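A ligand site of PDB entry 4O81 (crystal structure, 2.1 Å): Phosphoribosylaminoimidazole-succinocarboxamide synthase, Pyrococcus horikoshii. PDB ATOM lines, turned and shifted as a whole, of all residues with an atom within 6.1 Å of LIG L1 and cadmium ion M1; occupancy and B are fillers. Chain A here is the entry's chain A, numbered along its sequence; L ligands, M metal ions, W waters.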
ATOM      1  N   ALA A  12       8.320 -18.521  30.780  1.00  0.00           N
ATOM      2  CA  ALA A  12       7.516 -18.768  29.548  1.00  0.00           C
ATOM      3  C   ALA A  12       8.345 -19.313  28.388  1.00  0.00           C
ATOM      4  O   ALA A  12       7.799 -19.634  27.330  1.00  0.00           O
ATOM      5  CB  ALA A  12       6.765 -17.514  29.126  1.00  0.00           C
ATOM      6  N   LYS A  13       9.661 -19.387  28.593  1.00  0.00           N
ATOM      7  CA  LYS A  13      10.577 -20.079  27.668  1.00  0.00           C
ATOM      8  C   LYS A  13      11.497 -21.039  28.431  1.00  0.00           C
ATOM      9  O   LYS A  13      11.839 -20.804  29.602  1.00  0.00           O
ATOM     10  CB  LYS A  13      11.416 -19.092  26.844  1.00  0.00           C
ATOM     11  CG  LYS A  13      10.639 -18.090  25.999  1.00  0.00           C
ATOM     12  CD  LYS A  13      11.518 -17.434  24.947  1.00  0.00           C
ATOM     13  CE  LYS A  13      12.589 -16.545  25.558  1.00  0.00           C
ATOM     14  NZ  LYS A  13      12.007 -15.370  26.254  1.00  0.00           N
ATOM     15  N   LYS A  14      11.882 -22.115  27.766  1.00  0.00           N
ATOM     16  CA  LYS A  14      12.938 -22.998  28.251  1.00  0.00           C
ATOM     17  C   LYS A  14      14.086 -22.927  27.262  1.00  0.00           C
ATOM     18  O   LYS A  14      13.883 -23.017  26.052  1.00  0.00           O
ATOM     19  CB  LYS A  14      12.403 -24.430  28.363  1.00  0.00           C
ATOM     20  N   MET A  15      15.306 -22.737  27.775  1.00  0.00           N
ATOM     21  CA  MET A  15      16.504 -22.685  26.932  1.00  0.00           C
ATOM     22  C   MET A  15      17.246 -23.976  27.066  1.00  0.00           C
ATOM     23  O   MET A  15      17.828 -24.268  28.111  1.00  0.00           O
ATOM     24  CB  MET A  15      17.415 -21.516  27.284  1.00  0.00           C
ATOM     25  CG  MET A  15      16.687 -20.173  27.369  1.00  0.00           C
ATOM     26  SD  MET A  15      15.903 -19.667  25.629  1.00  0.00           S
ATOM     27  CE  MET A  15      17.513 -18.940  24.769  1.00  0.00           C
ATOM     28  N   LEU A  23      21.591 -23.351  20.699  1.00  0.00           N
ATOM     29  CA  LEU A  23      20.606 -23.840  21.660  1.00  0.00           C
ATOM     30  C   LEU A  23      19.179 -23.817  21.118  1.00  0.00           C
ATOM     31  O   LEU A  23      18.898 -23.239  20.062  1.00  0.00           O
ATOM     32  CB  LEU A  23      20.720 -23.075  22.981  1.00  0.00           C
ATOM     33  CG  LEU A  23      20.293 -21.625  23.044  1.00  0.00           C
ATOM     34  CD1 LEU A  23      18.945 -21.577  23.724  1.00  0.00           C
ATOM     35  CD2 LEU A  23      21.316 -20.800  23.811  1.00  0.00           C
ATOM     36  N   MET A  25      15.361 -22.700  21.951  1.00  0.00           N
ATOM     37  CA  MET A  25      14.503 -21.836  22.745  1.00  0.00           C
ATOM     38  C   MET A  25      13.128 -22.420  22.570  1.00  0.00           C
ATOM     39  O   MET A  25      12.563 -22.396  21.476  1.00  0.00           O
ATOM     40  CB  MET A  25      14.663 -20.427  22.157  1.00  0.00           C
ATOM     41  CG  MET A  25      13.655 -19.428  22.678  1.00  0.00           C
ATOM     42  SD  MET A  25      14.331 -17.611  22.286  1.00  0.00           S
ATOM     43  CE  MET A  25      13.941 -17.513  20.361  1.00  0.00           C
ATOM     44  N   HIS A  68      19.926 -13.838  16.476  1.00  0.00           N
ATOM     45  CA  HIS A  68      20.375 -15.156  16.914  1.00  0.00           C
ATOM     46  C   HIS A  68      19.644 -16.274  16.241  1.00  0.00           C
ATOM     47  O   HIS A  68      20.008 -17.444  16.394  1.00  0.00           O
ATOM     48  CB  HIS A  68      20.280 -15.276  18.437  1.00  0.00           C
ATOM     49  CG  HIS A  68      18.863 -15.301  18.996  1.00  0.00           C
ATOM     50  ND1 HIS A  68      18.575 -15.849  20.186  1.00  0.00           N
ATOM     51  CD2 HIS A  68      17.649 -14.853  18.469  1.00  0.00           C
ATOM     52  CE1 HIS A  68      17.251 -15.738  20.433  1.00  0.00           C
ATOM     53  NE2 HIS A  68      16.691 -15.120  19.380  1.00  0.00           N
ATOM     54  N   VAL A  80      18.637 -21.309  17.967  1.00  0.00           N
ATOM     55  CA  VAL A  80      19.259 -20.001  18.030  1.00  0.00           C
ATOM     56  C   VAL A  80      20.726 -20.132  18.382  1.00  0.00           C
ATOM     57  O   VAL A  80      21.129 -21.102  19.048  1.00  0.00           O
ATOM     58  CB  VAL A  80      18.561 -19.044  19.024  1.00  0.00           C
ATOM     59  CG1 VAL A  80      17.138 -18.725  18.571  1.00  0.00           C
ATOM     60  CG2 VAL A  80      18.572 -19.611  20.448  1.00  0.00           C
ATOM     61  N   GLU A  81      21.527 -19.181  17.939  1.00  0.00           N
ATOM     62  CA  GLU A  81      22.933 -19.238  18.263  1.00  0.00           C
ATOM     63  C   GLU A  81      23.171 -18.781  19.704  1.00  0.00           C
ATOM     64  O   GLU A  81      22.500 -17.865  20.190  1.00  0.00           O
ATOM     65  CB  GLU A  81      23.783 -18.486  17.235  1.00  0.00           C
ATOM     66  CG  GLU A  81      23.762 -16.979  17.309  1.00  0.00           C
ATOM     67  CD  GLU A  81      24.882 -16.361  16.483  1.00  0.00           C
ATOM     68  OE1 GLU A  81      24.589 -15.455  15.672  1.00  0.00           O
ATOM     69  OE2 GLU A  81      26.041 -16.796  16.633  1.00  0.00           O
ATOM     70  N   LYS A  82      24.079 -19.468  20.382  1.00  0.00           N
ATOM     71  CA  LYS A  82      24.394 -19.121  21.768  1.00  0.00           C
ATOM     72  C   LYS A  82      25.229 -17.855  21.830  1.00  0.00           C
ATOM     73  O   LYS A  82      26.209 -17.702  21.119  1.00  0.00           O
ATOM     74  CB  LYS A  82      25.104 -20.271  22.493  1.00  0.00           C
ATOM     75  CG  LYS A  82      24.937 -20.171  24.003  1.00  0.00           C
ATOM     76  CD  LYS A  82      25.505 -21.381  24.725  1.00  0.00           C
ATOM     77  CE  LYS A  82      26.979 -21.181  25.077  1.00  0.00           C
ATOM     78  N   LEU A  83      24.804 -16.936  22.694  1.00  0.00           N
ATOM     79  CA  LEU A  83      25.475 -15.655  22.808  1.00  0.00           C
ATOM     80  C   LEU A  83      25.922 -15.411  24.238  1.00  0.00           C
ATOM     81  O   LEU A  83      25.358 -15.965  25.188  1.00  0.00           O
ATOM     82  CB  LEU A  83      24.536 -14.509  22.366  1.00  0.00           C
ATOM     83  CG  LEU A  83      24.008 -14.494  20.947  1.00  0.00           C
ATOM     84  CD1 LEU A  83      22.985 -13.376  20.811  1.00  0.00           C
ATOM     85  CD2 LEU A  83      25.141 -14.333  19.943  1.00  0.00           C
ATOM     86  N   ASP A  84      26.939 -14.570  24.359  1.00  0.00           N
ATOM     87  CA  ASP A  84      27.347 -13.996  25.620  1.00  0.00           C
ATOM     88  C   ASP A  84      26.475 -12.750  25.853  1.00  0.00           C
ATOM     89  O   ASP A  84      26.742 -11.687  25.303  1.00  0.00           O
ATOM     90  CB  ASP A  84      28.838 -13.640  25.527  1.00  0.00           C
ATOM     91  CG  ASP A  84      29.358 -13.005  26.784  1.00  0.00           C
ATOM     92  OD1 ASP A  84      28.841 -13.313  27.880  1.00  0.00           O
ATOM     93  OD2 ASP A  84      30.306 -12.203  26.674  1.00  0.00           O
ATOM     94  N   MET A  85      25.418 -12.901  26.669  1.00  0.00           N
ATOM     95  CA  MET A  85      24.346 -11.902  26.788  1.00  0.00           C
ATOM     96  C   MET A  85      24.761 -10.675  27.547  1.00  0.00           C
ATOM     97  O   MET A  85      25.448 -10.760  28.562  1.00  0.00           O
ATOM     98  CB  MET A  85      23.133 -12.466  27.534  1.00  0.00           C
ATOM     99  CG  MET A  85      22.424 -13.639  26.849  1.00  0.00           C
ATOM    100  SD  MET A  85      21.746 -13.147  25.063  1.00  0.00           S
ATOM    101  CE  MET A  85      20.474 -11.777  25.673  1.00  0.00           C
ATOM    102  N   LYS A 122      19.187  -6.026  33.864  1.00  0.00           N
ATOM    103  CA  LYS A 122      18.443  -7.288  34.003  1.00  0.00           C
ATOM    104  C   LYS A 122      18.845  -7.979  35.296  1.00  0.00           C
ATOM    105  O   LYS A 122      19.903  -8.585  35.357  1.00  0.00           O
ATOM    106  CB  LYS A 122      18.670  -8.181  32.788  1.00  0.00           C
ATOM    107  CG  LYS A 122      17.578  -9.215  32.550  1.00  0.00           C
ATOM    108  CD  LYS A 122      17.792 -10.004  31.261  1.00  0.00           C
ATOM    109  CE  LYS A 122      16.519 -10.736  30.845  1.00  0.00           C
ATOM    110  NZ  LYS A 122      16.257 -11.985  31.624  1.00  0.00           N
ATOM    111  N   LYS A 175      10.556  -4.587  24.367  1.00  0.00           N
ATOM    112  CA  LYS A 175      11.829  -4.879  24.992  1.00  0.00           C
ATOM    113  C   LYS A 175      12.651  -5.795  24.088  1.00  0.00           C
ATOM    114  O   LYS A 175      12.114  -6.741  23.519  1.00  0.00           O
ATOM    115  CB  LYS A 175      11.661  -5.582  26.362  1.00  0.00           C
ATOM    116  CG  LYS A 175      12.979  -6.121  26.937  1.00  0.00           C
ATOM    117  CD  LYS A 175      12.873  -7.432  27.740  1.00  0.00           C
ATOM    118  CE  LYS A 175      12.116  -8.547  27.039  1.00  0.00           C
ATOM    119  NZ  LYS A 175      12.938  -9.780  26.847  1.00  0.00           N
ATOM    120  N   GLU A 177      16.641  -7.842  23.803  1.00  0.00           N
ATOM    121  CA  GLU A 177      17.860  -8.260  24.460  1.00  0.00           C
ATOM    122  C   GLU A 177      18.941  -8.530  23.422  1.00  0.00           C
ATOM    123  O   GLU A 177      18.645  -8.876  22.260  1.00  0.00           O
ATOM    124  CB  GLU A 177      17.602  -9.479  25.369  1.00  0.00           C
ATOM    125  CG  GLU A 177      16.581  -9.168  26.449  1.00  0.00           C
ATOM    126  CD  GLU A 177      16.343 -10.298  27.446  1.00  0.00           C
ATOM    127  OE1 GLU A 177      17.185 -11.205  27.580  1.00  0.00           O
ATOM    128  OE2 GLU A 177      15.304 -10.248  28.125  1.00  0.00           O
ATOM    129  N   LEU A 188      21.155  -9.456  18.094  1.00  0.00           N
ATOM    130  CA  LEU A 188      19.797  -9.440  18.664  1.00  0.00           C
ATOM    131  C   LEU A 188      19.339 -10.853  19.079  1.00  0.00           C
ATOM    132  O   LEU A 188      19.474 -11.812  18.311  1.00  0.00           O
ATOM    133  CB  LEU A 188      18.811  -8.804  17.688  1.00  0.00           C
ATOM    134  CG  LEU A 188      17.343  -8.653  18.109  1.00  0.00           C
ATOM    135  CD1 LEU A 188      17.233  -7.773  19.354  1.00  0.00           C
ATOM    136  CD2 LEU A 188      16.538  -8.076  16.966  1.00  0.00           C
ATOM    137  N   ALA A 189      18.791 -10.963  20.275  1.00  0.00           N
ATOM    138  CA  ALA A 189      18.491 -12.272  20.849  1.00  0.00           C
ATOM    139  C   ALA A 189      17.077 -12.351  21.454  1.00  0.00           C
ATOM    140  O   ALA A 189      16.197 -11.579  21.096  1.00  0.00           O
ATOM    141  CB  ALA A 189      19.531 -12.615  21.895  1.00  0.00           C
ATOM    142  N   ASP A 190      16.921 -13.301  22.380  1.00  0.00           N
ATOM    143  CA  ASP A 190      15.661 -13.552  23.110  1.00  0.00           C
ATOM    144  C   ASP A 190      14.469 -13.721  22.159  1.00  0.00           C
ATOM    145  O   ASP A 190      14.571 -14.452  21.170  1.00  0.00           O
ATOM    146  CB  ASP A 190      15.425 -12.479  24.188  1.00  0.00           C
ATOM    147  CG  ASP A 190      14.418 -12.915  25.233  1.00  0.00           C
ATOM    148  OD1 ASP A 190      13.346 -12.277  25.360  1.00  0.00           O
ATOM    149  OD2 ASP A 190      14.688 -13.880  25.968  1.00  0.00           O
ATOM    150  N   GLU A 191      13.341 -13.065  22.450  1.00  0.00           N
ATOM    151  CA  GLU A 191      12.124 -13.214  21.631  1.00  0.00           C
ATOM    152  C   GLU A 191      11.580 -11.866  21.182  1.00  0.00           C
ATOM    153  O   GLU A 191      11.967 -10.833  21.712  1.00  0.00           O
ATOM    154  CB  GLU A 191      11.040 -13.998  22.384  1.00  0.00           C
ATOM    155  CG  GLU A 191      10.367 -13.205  23.479  1.00  0.00           C
ATOM    156  CD  GLU A 191       9.366 -14.014  24.272  1.00  0.00           C
ATOM    157  OE1 GLU A 191       8.262 -14.292  23.768  1.00  0.00           O
ATOM    158  OE2 GLU A 191       9.674 -14.342  25.428  1.00  0.00           O
HETATM  159  P1  LIG L   1      13.102 -16.599  30.051  1.00  0.00           P
HETATM  160  O1  LIG L   1      11.957 -17.256  29.314  1.00  0.00           O
HETATM  161  O2  LIG L   1      13.824 -17.528  30.994  1.00  0.00           O
HETATM  162  O3  LIG L   1      12.759 -15.275  30.694  1.00  0.00           O
HETATM  163  O4  LIG L   1      14.185 -16.208  28.917  1.00  0.00           O
HETATM  164  C1  LIG L   1      15.187 -17.126  28.467  1.00  0.00           C
HETATM  165  C2  LIG L   1      16.600 -16.706  28.882  1.00  0.00           C
HETATM  166  O5  LIG L   1      17.523 -16.966  27.813  1.00  0.00           O
HETATM  167  C3  LIG L   1      16.761 -15.227  29.218  1.00  0.00           C
HETATM  168  O6  LIG L   1      17.620 -15.149  30.351  1.00  0.00           O
HETATM  169  C4  LIG L   1      17.491 -14.651  28.023  1.00  0.00           C
HETATM  170  O7  LIG L   1      18.333 -13.549  28.391  1.00  0.00           O
HETATM  171  C5  LIG L   1      18.329 -15.817  27.562  1.00  0.00           C
HETATM  172  N1  LIG L   1      18.666 -15.775  26.126  1.00  0.00           N
HETATM  173  C6  LIG L   1      17.865 -15.349  25.142  1.00  0.00           C
HETATM  174  N2  LIG L   1      18.470 -15.474  23.954  1.00  0.00           N
HETATM  175  C7  LIG L   1      19.687 -16.007  24.170  1.00  0.00           C
HETATM  176  C8  LIG L   1      20.851 -16.412  23.335  1.00  0.00           C
HETATM  177  N3  LIG L   1      20.822 -16.258  22.003  1.00  0.00           N
HETATM  178  N4  LIG L   1      21.938 -16.929  23.956  1.00  0.00           N
HETATM  179  C9  LIG L   1      21.993 -17.096  25.294  1.00  0.00           C
HETATM  180  N5  LIG L   1      20.968 -16.758  26.105  1.00  0.00           N
HETATM  181  C10 LIG L   1      19.822 -16.213  25.608  1.00  0.00           C
HETATM  182  P1  LG2 L   2       7.014  -0.930  30.977  1.00  0.00           P
HETATM  183  O1  LG2 L   2       8.374  -0.400  31.370  1.00  0.00           O
HETATM  184  O2  LG2 L   2       6.050   0.124  30.506  1.00  0.00           O
HETATM  185  O3  LG2 L   2       6.381  -1.849  31.989  1.00  0.00           O
HETATM  186  O4  LG2 L   2       7.323  -1.919  29.710  1.00  0.00           O
HETATM  187  C1  LG2 L   2       7.729  -1.433  28.418  1.00  0.00           C
HETATM  188  C2  LG2 L   2       7.690  -2.485  27.280  1.00  0.00           C
HETATM  189  O5  LG2 L   2       8.778  -3.410  27.383  1.00  0.00           O
HETATM  190  C3  LG2 L   2       6.444  -3.366  27.228  1.00  0.00           C
HETATM  191  O6  LG2 L   2       6.151  -3.706  25.870  1.00  0.00           O
HETATM  192  C4  LG2 L   2       6.832  -4.629  27.948  1.00  0.00           C
HETATM  193  O7  LG2 L   2       6.083  -5.758  27.488  1.00  0.00           O
HETATM  194  C5  LG2 L   2       8.315  -4.745  27.619  1.00  0.00           C
HETATM  195  N1  LG2 L   2       9.042  -5.370  28.746  1.00  0.00           N
HETATM  196  C6  LG2 L   2       9.660  -4.737  29.757  1.00  0.00           C
HETATM  197  N2  LG2 L   2      10.217  -5.626  30.620  1.00  0.00           N
HETATM  198  C7  LG2 L   2       9.956  -6.851  30.183  1.00  0.00           C
HETATM  199  C8  LG2 L   2      10.242  -8.247  30.631  1.00  0.00           C
HETATM  200  N3  LG2 L   2      10.950  -8.497  31.757  1.00  0.00           N
HETATM  201  N4  LG2 L   2       9.770  -9.260  29.852  1.00  0.00           N
HETATM  202  C9  LG2 L   2       9.068  -9.029  28.725  1.00  0.00           C
HETATM  203  N5  LG2 L   2       8.766  -7.797  28.263  1.00  0.00           N
HETATM  204  C10 LG2 L   2       9.172  -6.687  28.933  1.00  0.00           C
HETATM  205 CD    CD M   1      12.552 -13.281  29.611  1.00  0.00          CD
HETATM  206 CD    CD M   2      10.165 -11.585  30.372  1.00  0.00          CD
HETATM  207 CD    CD M   3      13.251  -9.076  33.910  1.00  0.00          CD
HETATM  208  O   HOH W   1      10.041 -14.105  30.574  1.00  0.00           O
HETATM  209  O   HOH W   2      11.155 -12.200  27.684  1.00  0.00           O
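OE1 of Glu 177 is in hydrogen-bond range of O7 of LIG L1, 2.7 Å away.
A ring nitrogen (ND1) of His 68 lies within hydrogen-bond range of a nitrogen (N3) of LIG L1 (2.9 Å).
O of Glu 81 lies within hydrogen-bond range of N3 of LIG L1.
The backbone NH (N) of Asp 190 is in hydrogen-bond range of a nitrogen (N2) of LIG L1, at 3.1 Å.
The backbone NH (N) of Lys 13 lies close to an oxygen (O1) of LIG L1 (3.2 Å).
NZ of Lys 13 is in salt-bridge range of O1 of LIG L1, 3.6 Å away.
N4 of LIG L1 is in hydrogen-bond range of N of Leu 83 (3.1 Å).
O of Glu 177 is in hydrogen-bond range of N of Ala 189, 2.9 Å away.
The side-chain carboxylate (OE2) of Glu 177 is in salt-bridge range of the side-chain amino group (NZ) of Lys 175 (2.7 Å).
The backbone NH (N) of Glu 81 is in hydrogen-bond range of the backbone carbonyl oxygen (O) of His 68.
The backbone carbonyl oxygen (O) of Asp 190 lies within hydrogen-bond range of a ring nitrogen (NE2) of His 68.
The backbone NH of His 68 lies within hydrogen-bond range of the backbone carbonyl oxygen of Leu 188 (2.8 Å).
The side-chain amino group of Lys 13 is in salt-bridge range of the side-chain carboxylate of Asp 190.
OE2 of Glu 191 is in salt-bridge range of NZ of Lys 13.
N of Leu 23 is in hydrogen-bond range of O of Val 80 (2.8 Å).
CG of Met 15 touches O5 of LIG L1 (3.3 Å).
Leu 23 touches LIG L1.
CA of Lys 82 touches N4 of LIG L1, 3.95 Å away.
Met 85 touches LIG L1 (CG to N5, 3.5 Å).
Lys 122 touches LIG L1.
Ala 189 touches LIG L1 (CB to N2, 3.7 Å).
Hydrophobic or aromatic side chains that line LIG L1: Met 15, Leu 23, His 68, Leu 83, Met 85 and Ala 189.
Within 4 Å of LIG L1: Lys 13, Met 15, Leu 23, His 68, Glu 81, Lys 82, Leu 83, Met 85, Lys 122, Glu 177, Ala 189 and Asp 190.
The nearest printed residue that does not touch LIG L1 is Ala 12 (4.1 Å).
Residues that only touch cadmium ion M1: Lys 13 (3.99 Å).
Of the 20 residues printed, 1 comes within 4 Å of cadmium ion M1.
Cadmium ion M1 is bound by O3 of LIG L1 (2.3 Å).
Slightly farther from cadmium ion M1 lies water W2 (2.6 Å).
Slightly farther from cadmium ion M1 lies water W1 (2.8 Å).
Water W2 lies within hydrogen-bond range of the side-chain amino group (NZ) of Lys 175 (3.1 Å), the side-chain carboxylate (OD1) of Asp 190 (3.2 Å) and the side-chain carboxylate (OE2) of Glu 191 (3.4 Å).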
